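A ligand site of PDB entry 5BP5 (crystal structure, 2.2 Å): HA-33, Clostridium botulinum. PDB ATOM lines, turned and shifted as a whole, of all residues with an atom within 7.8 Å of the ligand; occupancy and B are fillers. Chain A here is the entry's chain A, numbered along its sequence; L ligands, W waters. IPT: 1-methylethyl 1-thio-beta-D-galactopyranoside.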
ATOM      1  N   ASN A 220       5.485  17.021   5.814  1.00  0.00           N
ATOM      2  CA  ASN A 220       5.388  18.490   5.916  1.00  0.00           C
ATOM      3  C   ASN A 220       5.906  19.246   4.696  1.00  0.00           C
ATOM      4  O   ASN A 220       6.077  20.469   4.748  1.00  0.00           O
ATOM      5  CB  ASN A 220       6.183  18.986   7.121  1.00  0.00           C
ATOM      6  CG  ASN A 220       5.735  18.360   8.425  1.00  0.00           C
ATOM      7  OD1 ASN A 220       4.542  18.222   8.681  1.00  0.00           O
ATOM      8  ND2 ASN A 220       6.684  17.991   9.260  1.00  0.00           N
ATOM      9  N   ALA A 260       1.467  25.327  10.187  1.00  0.00           N
ATOM     10  CA  ALA A 260       1.924  26.680   9.847  1.00  0.00           C
ATOM     11  C   ALA A 260       3.053  26.645   8.834  1.00  0.00           C
ATOM     12  O   ALA A 260       3.858  25.725   8.830  1.00  0.00           O
ATOM     13  CB  ALA A 260       2.382  27.411  11.089  1.00  0.00           C
ATOM     14  N   LEU A 261       3.128  27.674   8.017  1.00  0.00           N
ATOM     15  CA  LEU A 261       4.300  27.840   7.155  1.00  0.00           C
ATOM     16  C   LEU A 261       5.500  28.018   8.088  1.00  0.00           C
ATOM     17  O   LEU A 261       5.468  28.853   8.989  1.00  0.00           O
ATOM     18  CB  LEU A 261       4.148  29.019   6.196  1.00  0.00           C
ATOM     19  CG  LEU A 261       5.111  28.999   5.001  1.00  0.00           C
ATOM     20  CD1 LEU A 261       4.744  27.896   3.997  1.00  0.00           C
ATOM     21  CD2 LEU A 261       5.124  30.345   4.313  1.00  0.00           C
ATOM     22  N   ASP A 262       6.528  27.214   7.844  1.00  0.00           N
ATOM     23  CA  ASP A 262       7.619  27.039   8.786  1.00  0.00           C
ATOM     24  C   ASP A 262       8.971  26.965   8.064  1.00  0.00           C
ATOM     25  O   ASP A 262       9.171  26.154   7.145  1.00  0.00           O
ATOM     26  CB  ASP A 262       7.359  25.770   9.605  1.00  0.00           C
ATOM     27  CG  ASP A 262       8.479  25.424  10.557  1.00  0.00           C
ATOM     28  OD1 ASP A 262       8.263  25.492  11.792  1.00  0.00           O
ATOM     29  OD2 ASP A 262       9.559  25.019  10.064  1.00  0.00           O
ATOM     30  N   LEU A 263       9.896  27.829   8.486  1.00  0.00           N
ATOM     31  CA  LEU A 263      11.273  27.792   8.031  1.00  0.00           C
ATOM     32  C   LEU A 263      12.011  26.694   8.799  1.00  0.00           C
ATOM     33  O   LEU A 263      12.072  26.727  10.038  1.00  0.00           O
ATOM     34  CB  LEU A 263      11.942  29.151   8.255  1.00  0.00           C
ATOM     35  CG  LEU A 263      13.410  29.295   7.864  1.00  0.00           C
ATOM     36  CD1 LEU A 263      13.647  29.023   6.386  1.00  0.00           C
ATOM     37  CD2 LEU A 263      13.876  30.692   8.222  1.00  0.00           C
ATOM     38  N   TYR A 264      12.548  25.735   8.053  1.00  0.00           N
ATOM     39  CA  TYR A 264      13.111  24.526   8.609  1.00  0.00           C
ATOM     40  C   TYR A 264      14.255  24.820   9.580  1.00  0.00           C
ATOM     41  O   TYR A 264      15.285  25.381   9.194  1.00  0.00           O
ATOM     42  CB  TYR A 264      13.605  23.597   7.489  1.00  0.00           C
ATOM     43  CG  TYR A 264      14.083  22.261   7.980  1.00  0.00           C
ATOM     44  CD1 TYR A 264      13.202  21.198   8.152  1.00  0.00           C
ATOM     45  CD2 TYR A 264      15.422  22.056   8.294  1.00  0.00           C
ATOM     46  CE1 TYR A 264      13.641  19.968   8.621  1.00  0.00           C
ATOM     47  CE2 TYR A 264      15.882  20.833   8.757  1.00  0.00           C
ATOM     48  CZ  TYR A 264      14.984  19.797   8.920  1.00  0.00           C
ATOM     49  OH  TYR A 264      15.422  18.577   9.380  1.00  0.00           O
ATOM     50  N   GLY A 265      14.028  24.450  10.839  1.00  0.00           N
ATOM     51  CA  GLY A 265      15.040  24.567  11.882  1.00  0.00           C
ATOM     52  C   GLY A 265      15.401  25.987  12.296  1.00  0.00           C
ATOM     53  O   GLY A 265      16.344  26.181  13.062  1.00  0.00           O
ATOM     54  N   GLY A 266      14.665  26.975  11.809  1.00  0.00           N
ATOM     55  CA  GLY A 266      15.078  28.364  11.940  1.00  0.00           C
ATOM     56  C   GLY A 266      16.398  28.670  11.229  1.00  0.00           C
ATOM     57  O   GLY A 266      17.049  29.665  11.549  1.00  0.00           O
ATOM     58  N   GLN A 267      16.769  27.836  10.245  1.00  0.00           N
ATOM     59  CA  GLN A 267      18.026  28.006   9.522  1.00  0.00           C
ATOM     60  C   GLN A 267      17.780  29.030   8.431  1.00  0.00           C
ATOM     61  O   GLN A 267      16.754  29.001   7.758  1.00  0.00           O
ATOM     62  CB  GLN A 267      18.515  26.705   8.880  1.00  0.00           C
ATOM     63  CG  GLN A 267      18.630  25.495   9.807  1.00  0.00           C
ATOM     64  CD  GLN A 267      19.634  25.688  10.922  1.00  0.00           C
ATOM     65  OE1 GLN A 267      20.449  26.610  10.901  1.00  0.00           O
ATOM     66  NE2 GLN A 267      19.591  24.811  11.911  1.00  0.00           N
ATOM     67  N   ALA A 273      14.866  24.464   3.698  1.00  0.00           N
ATOM     68  CA  ALA A 273      13.521  24.064   3.281  1.00  0.00           C
ATOM     69  C   ALA A 273      12.419  24.948   3.883  1.00  0.00           C
ATOM     70  O   ALA A 273      12.472  25.343   5.051  1.00  0.00           O
ATOM     71  CB  ALA A 273      13.263  22.606   3.640  1.00  0.00           C
ATOM     72  N   GLN A 275       8.522  24.567   4.784  1.00  0.00           N
ATOM     73  CA  GLN A 275       7.605  23.464   5.026  1.00  0.00           C
ATOM     74  C   GLN A 275       6.362  23.930   5.775  1.00  0.00           C
ATOM     75  O   GLN A 275       6.178  25.125   6.016  1.00  0.00           O
ATOM     76  CB  GLN A 275       8.300  22.363   5.797  1.00  0.00           C
ATOM     77  CG  GLN A 275       8.792  22.777   7.171  1.00  0.00           C
ATOM     78  CD  GLN A 275       9.403  21.638   7.942  1.00  0.00           C
ATOM     79  OE1 GLN A 275       9.634  20.549   7.397  1.00  0.00           O
ATOM     80  NE2 GLN A 275       9.673  21.872   9.218  1.00  0.00           N
ATOM     81  N   VAL A 276       5.491  22.992   6.113  1.00  0.00           N
ATOM     82  CA  VAL A 276       4.492  23.215   7.147  1.00  0.00           C
ATOM     83  C   VAL A 276       4.972  22.546   8.427  1.00  0.00           C
ATOM     84  O   VAL A 276       5.865  21.690   8.377  1.00  0.00           O
ATOM     85  CB  VAL A 276       3.086  22.708   6.764  1.00  0.00           C
ATOM     86  CG1 VAL A 276       2.550  23.519   5.588  1.00  0.00           C
ATOM     87  CG2 VAL A 276       3.085  21.215   6.466  1.00  0.00           C
ATOM     88  N   PHE A 277       4.404  22.931   9.565  1.00  0.00           N
ATOM     89  CA  PHE A 277       4.759  22.316  10.851  1.00  0.00           C
ATOM     90  C   PHE A 277       3.730  22.728  11.908  1.00  0.00           C
ATOM     91  O   PHE A 277       3.112  23.782  11.802  1.00  0.00           O
ATOM     92  CB  PHE A 277       6.183  22.718  11.293  1.00  0.00           C
ATOM     93  CG  PHE A 277       6.732  21.913  12.452  1.00  0.00           C
ATOM     94  CD1 PHE A 277       7.423  20.723  12.233  1.00  0.00           C
ATOM     95  CD2 PHE A 277       6.596  22.360  13.769  1.00  0.00           C
ATOM     96  CE1 PHE A 277       7.940  19.991  13.294  1.00  0.00           C
ATOM     97  CE2 PHE A 277       7.108  21.636  14.842  1.00  0.00           C
ATOM     98  CZ  PHE A 277       7.782  20.441  14.608  1.00  0.00           C
ATOM     99  N   ASN A 278       3.533  21.884  12.916  1.00  0.00           N
ATOM    100  CA  ASN A 278       2.619  22.191  14.030  1.00  0.00           C
ATOM    101  C   ASN A 278       2.810  23.654  14.523  1.00  0.00           C
ATOM    102  O   ASN A 278       3.941  24.085  14.762  1.00  0.00           O
ATOM    103  CB  ASN A 278       2.844  21.179  15.151  1.00  0.00           C
ATOM    104  CG  ASN A 278       1.936  21.406  16.346  1.00  0.00           C
ATOM    105  OD1 ASN A 278       2.402  21.452  17.486  1.00  0.00           O
ATOM    106  ND2 ASN A 278       0.646  21.547  16.093  1.00  0.00           N
ATOM    107  N   TYR A 279       1.721  24.408  14.635  1.00  0.00           N
ATOM    108  CA  TYR A 279       1.797  25.826  14.987  1.00  0.00           C
ATOM    109  C   TYR A 279       2.223  26.052  16.434  1.00  0.00           C
ATOM    110  O   TYR A 279       1.531  25.636  17.355  1.00  0.00           O
ATOM    111  CB  TYR A 279       0.463  26.553  14.752  1.00  0.00           C
ATOM    112  CG  TYR A 279       0.501  27.999  15.235  1.00  0.00           C
ATOM    113  CD1 TYR A 279       1.013  29.021  14.434  1.00  0.00           C
ATOM    114  CD2 TYR A 279       0.049  28.345  16.521  1.00  0.00           C
ATOM    115  CE1 TYR A 279       1.067  30.338  14.880  1.00  0.00           C
ATOM    116  CE2 TYR A 279       0.103  29.650  16.985  1.00  0.00           C
ATOM    117  CZ  TYR A 279       0.607  30.639  16.168  1.00  0.00           C
ATOM    118  OH  TYR A 279       0.656  31.933  16.619  1.00  0.00           O
ATOM    119  N   HIS A 280       3.356  26.732  16.608  1.00  0.00           N
ATOM    120  CA  HIS A 280       3.821  27.162  17.939  1.00  0.00           C
ATOM    121  C   HIS A 280       4.061  28.676  18.058  1.00  0.00           C
ATOM    122  O   HIS A 280       4.275  29.193  19.151  1.00  0.00           O
ATOM    123  CB  HIS A 280       5.092  26.397  18.362  1.00  0.00           C
ATOM    124  CG  HIS A 280       6.149  26.322  17.299  1.00  0.00           C
ATOM    125  ND1 HIS A 280       6.511  27.399  16.520  1.00  0.00           N
ATOM    126  CD2 HIS A 280       6.945  25.298  16.908  1.00  0.00           C
ATOM    127  CE1 HIS A 280       7.470  27.049  15.686  1.00  0.00           C
ATOM    128  NE2 HIS A 280       7.747  25.768  15.902  1.00  0.00           N
ATOM    129  N   GLY A 281       4.029  29.402  16.939  1.00  0.00           N
ATOM    130  CA  GLY A 281       4.195  30.849  16.952  1.00  0.00           C
ATOM    131  C   GLY A 281       5.580  31.372  17.313  1.00  0.00           C
ATOM    132  O   GLY A 281       5.705  32.515  17.724  1.00  0.00           O
ATOM    133  N   ASP A 282       6.603  30.547  17.168  1.00  0.00           N
ATOM    134  CA  ASP A 282       7.984  31.005  17.302  1.00  0.00           C
ATOM    135  C   ASP A 282       8.352  31.810  16.063  1.00  0.00           C
ATOM    136  O   ASP A 282       7.560  31.894  15.100  1.00  0.00           O
ATOM    137  CB  ASP A 282       8.955  29.820  17.443  1.00  0.00           C
ATOM    138  CG  ASP A 282       8.682  28.983  18.684  1.00  0.00           C
ATOM    139  OD1 ASP A 282       8.215  29.551  19.693  1.00  0.00           O
ATOM    140  OD2 ASP A 282       8.953  27.765  18.652  1.00  0.00           O
ATOM    141  N   ASN A 284      10.371  31.388  13.580  1.00  0.00           N
ATOM    142  CA  ASN A 284      10.491  30.691  12.294  1.00  0.00           C
ATOM    143  C   ASN A 284       9.137  30.284  11.689  1.00  0.00           C
ATOM    144  O   ASN A 284       9.080  29.554  10.705  1.00  0.00           O
ATOM    145  CB  ASN A 284      11.416  29.472  12.400  1.00  0.00           C
ATOM    146  CG  ASN A 284      10.798  28.324  13.173  1.00  0.00           C
ATOM    147  OD1 ASN A 284      10.252  28.511  14.243  1.00  0.00           O
ATOM    148  ND2 ASN A 284      10.884  27.125  12.616  1.00  0.00           N
ATOM    149  N   GLN A 285       8.046  30.738  12.300  1.00  0.00           N
ATOM    150  CA  GLN A 285       6.716  30.634  11.704  1.00  0.00           C
ATOM    151  C   GLN A 285       6.129  32.034  11.512  1.00  0.00           C
ATOM    152  O   GLN A 285       4.905  32.201  11.449  1.00  0.00           O
ATOM    153  CB  GLN A 285       5.803  29.750  12.576  1.00  0.00           C
ATOM    154  CG  GLN A 285       6.278  28.309  12.701  1.00  0.00           C
ATOM    155  CD  GLN A 285       5.345  27.411  13.537  1.00  0.00           C
ATOM    156  OE1 GLN A 285       4.470  27.882  14.261  1.00  0.00           O
ATOM    157  NE2 GLN A 285       5.566  26.099  13.430  1.00  0.00           N
HETATM  158  C1  IPT L   1      12.577  22.898  14.975  1.00  0.00           C
HETATM  159  C2  IPT L   1      11.546  24.003  14.925  1.00  0.00           C
HETATM  160  O2  IPT L   1      11.243  24.468  16.245  1.00  0.00           O
HETATM  161  C3  IPT L   1      10.252  23.583  14.216  1.00  0.00           C
HETATM  162  O3  IPT L   1       9.439  24.759  14.051  1.00  0.00           O
HETATM  163  C4  IPT L   1      10.581  22.949  12.864  1.00  0.00           C
HETATM  164  O4  IPT L   1      11.042  23.995  11.976  1.00  0.00           O
HETATM  165  C5  IPT L   1      11.634  21.851  13.043  1.00  0.00           C
HETATM  166  O5  IPT L   1      12.815  22.381  13.635  1.00  0.00           O
HETATM  167  C6  IPT L   1      12.008  21.155  11.721  1.00  0.00           C
HETATM  168  O6  IPT L   1      10.862  20.455  11.253  1.00  0.00           O
HETATM  169  S1  IPT L   1      14.091  23.540  15.645  1.00  0.00           S
HETATM  170  C1' IPT L   1      15.132  22.113  15.566  1.00  0.00           C
HETATM  171  C2' IPT L   1      16.571  22.424  16.017  1.00  0.00           C
HETATM  172  C3' IPT L   1      14.483  20.984  16.356  1.00  0.00           C
HETATM  173  O   HOH W   1      11.219  27.167  16.547  1.00  0.00           O
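The backbone carbonyl oxygen (O) of Gln 275 sits at hydrogen-bond distance from the backbone NH (N) of Asp 262 (2.8 Å). The side-chain carboxylate (OD1) of Asp 262 is in hydrogen-bond range of the side-chain amide nitrogen (ND2) of Asn 284 (3.2 Å). The side-chain carboxylate (OD1) of Asp 262 sits at hydrogen-bond distance from the side-chain amide nitrogen (NE2) of Gln 285 (3.2 Å). The backbone NH of His 280 sits at hydrogen-bond distance from the side-chain amide oxygen of Gln 285, at 2.8 Å. The backbone NH (N) of Asp 282 is in hydrogen-bond range of a ring nitrogen (ND1) of His 280, at 3.2 Å. The side-chain amide nitrogen (ND2) of Asn 284 sits at hydrogen-bond distance from the backbone carbonyl oxygen (O) of Leu 263, 2.9 Å away. The backbone carbonyl oxygen of Phe 277 sits at hydrogen-bond distance from the backbone NH of Ala 260, 2.8 Å away. The backbone NH of Tyr 264 sits at hydrogen-bond distance from the backbone carbonyl oxygen of Ala 273, at 3.0 Å.
Water W1 lies within hydrogen-bond range of an oxygen (O2) of the ligand, the side-chain amide oxygen (OD1) of Asn 284 and the side-chain carboxylate (OD2) of Asp 282.
The side-chain carboxylate (OD2) of Asp 262 lies within hydrogen-bond range of an oxygen (O4) of the ligand, at 2.6 Å. O3 of the ligand lies within hydrogen-bond range of NE2 of His 280 (2.7 Å). The side-chain amide nitrogen (NE2) of Gln 275 sits at hydrogen-bond distance from an oxygen (O6) of the ligand (2.8 Å). An oxygen (O3) of the ligand is in hydrogen-bond range of the side-chain amide nitrogen (ND2) of Asn 284. The backbone NH of Gly 265 is in hydrogen-bond range of an oxygen (O4) of the ligand (3.2 Å).
Merely in contact with the ligand: Leu 263 (3.5 Å), Tyr 264 (3.7 Å) and Phe 277 (3.6 Å). Hydrophobic or aromatic side chains within 4 Å of the ligand: Tyr 264, Phe 277 and His 280. Of the 20 residues printed, 8 come within 4 Å of the ligand. The nearest printed residue that does not touch the ligand is Gln 285 (4.1 Å).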
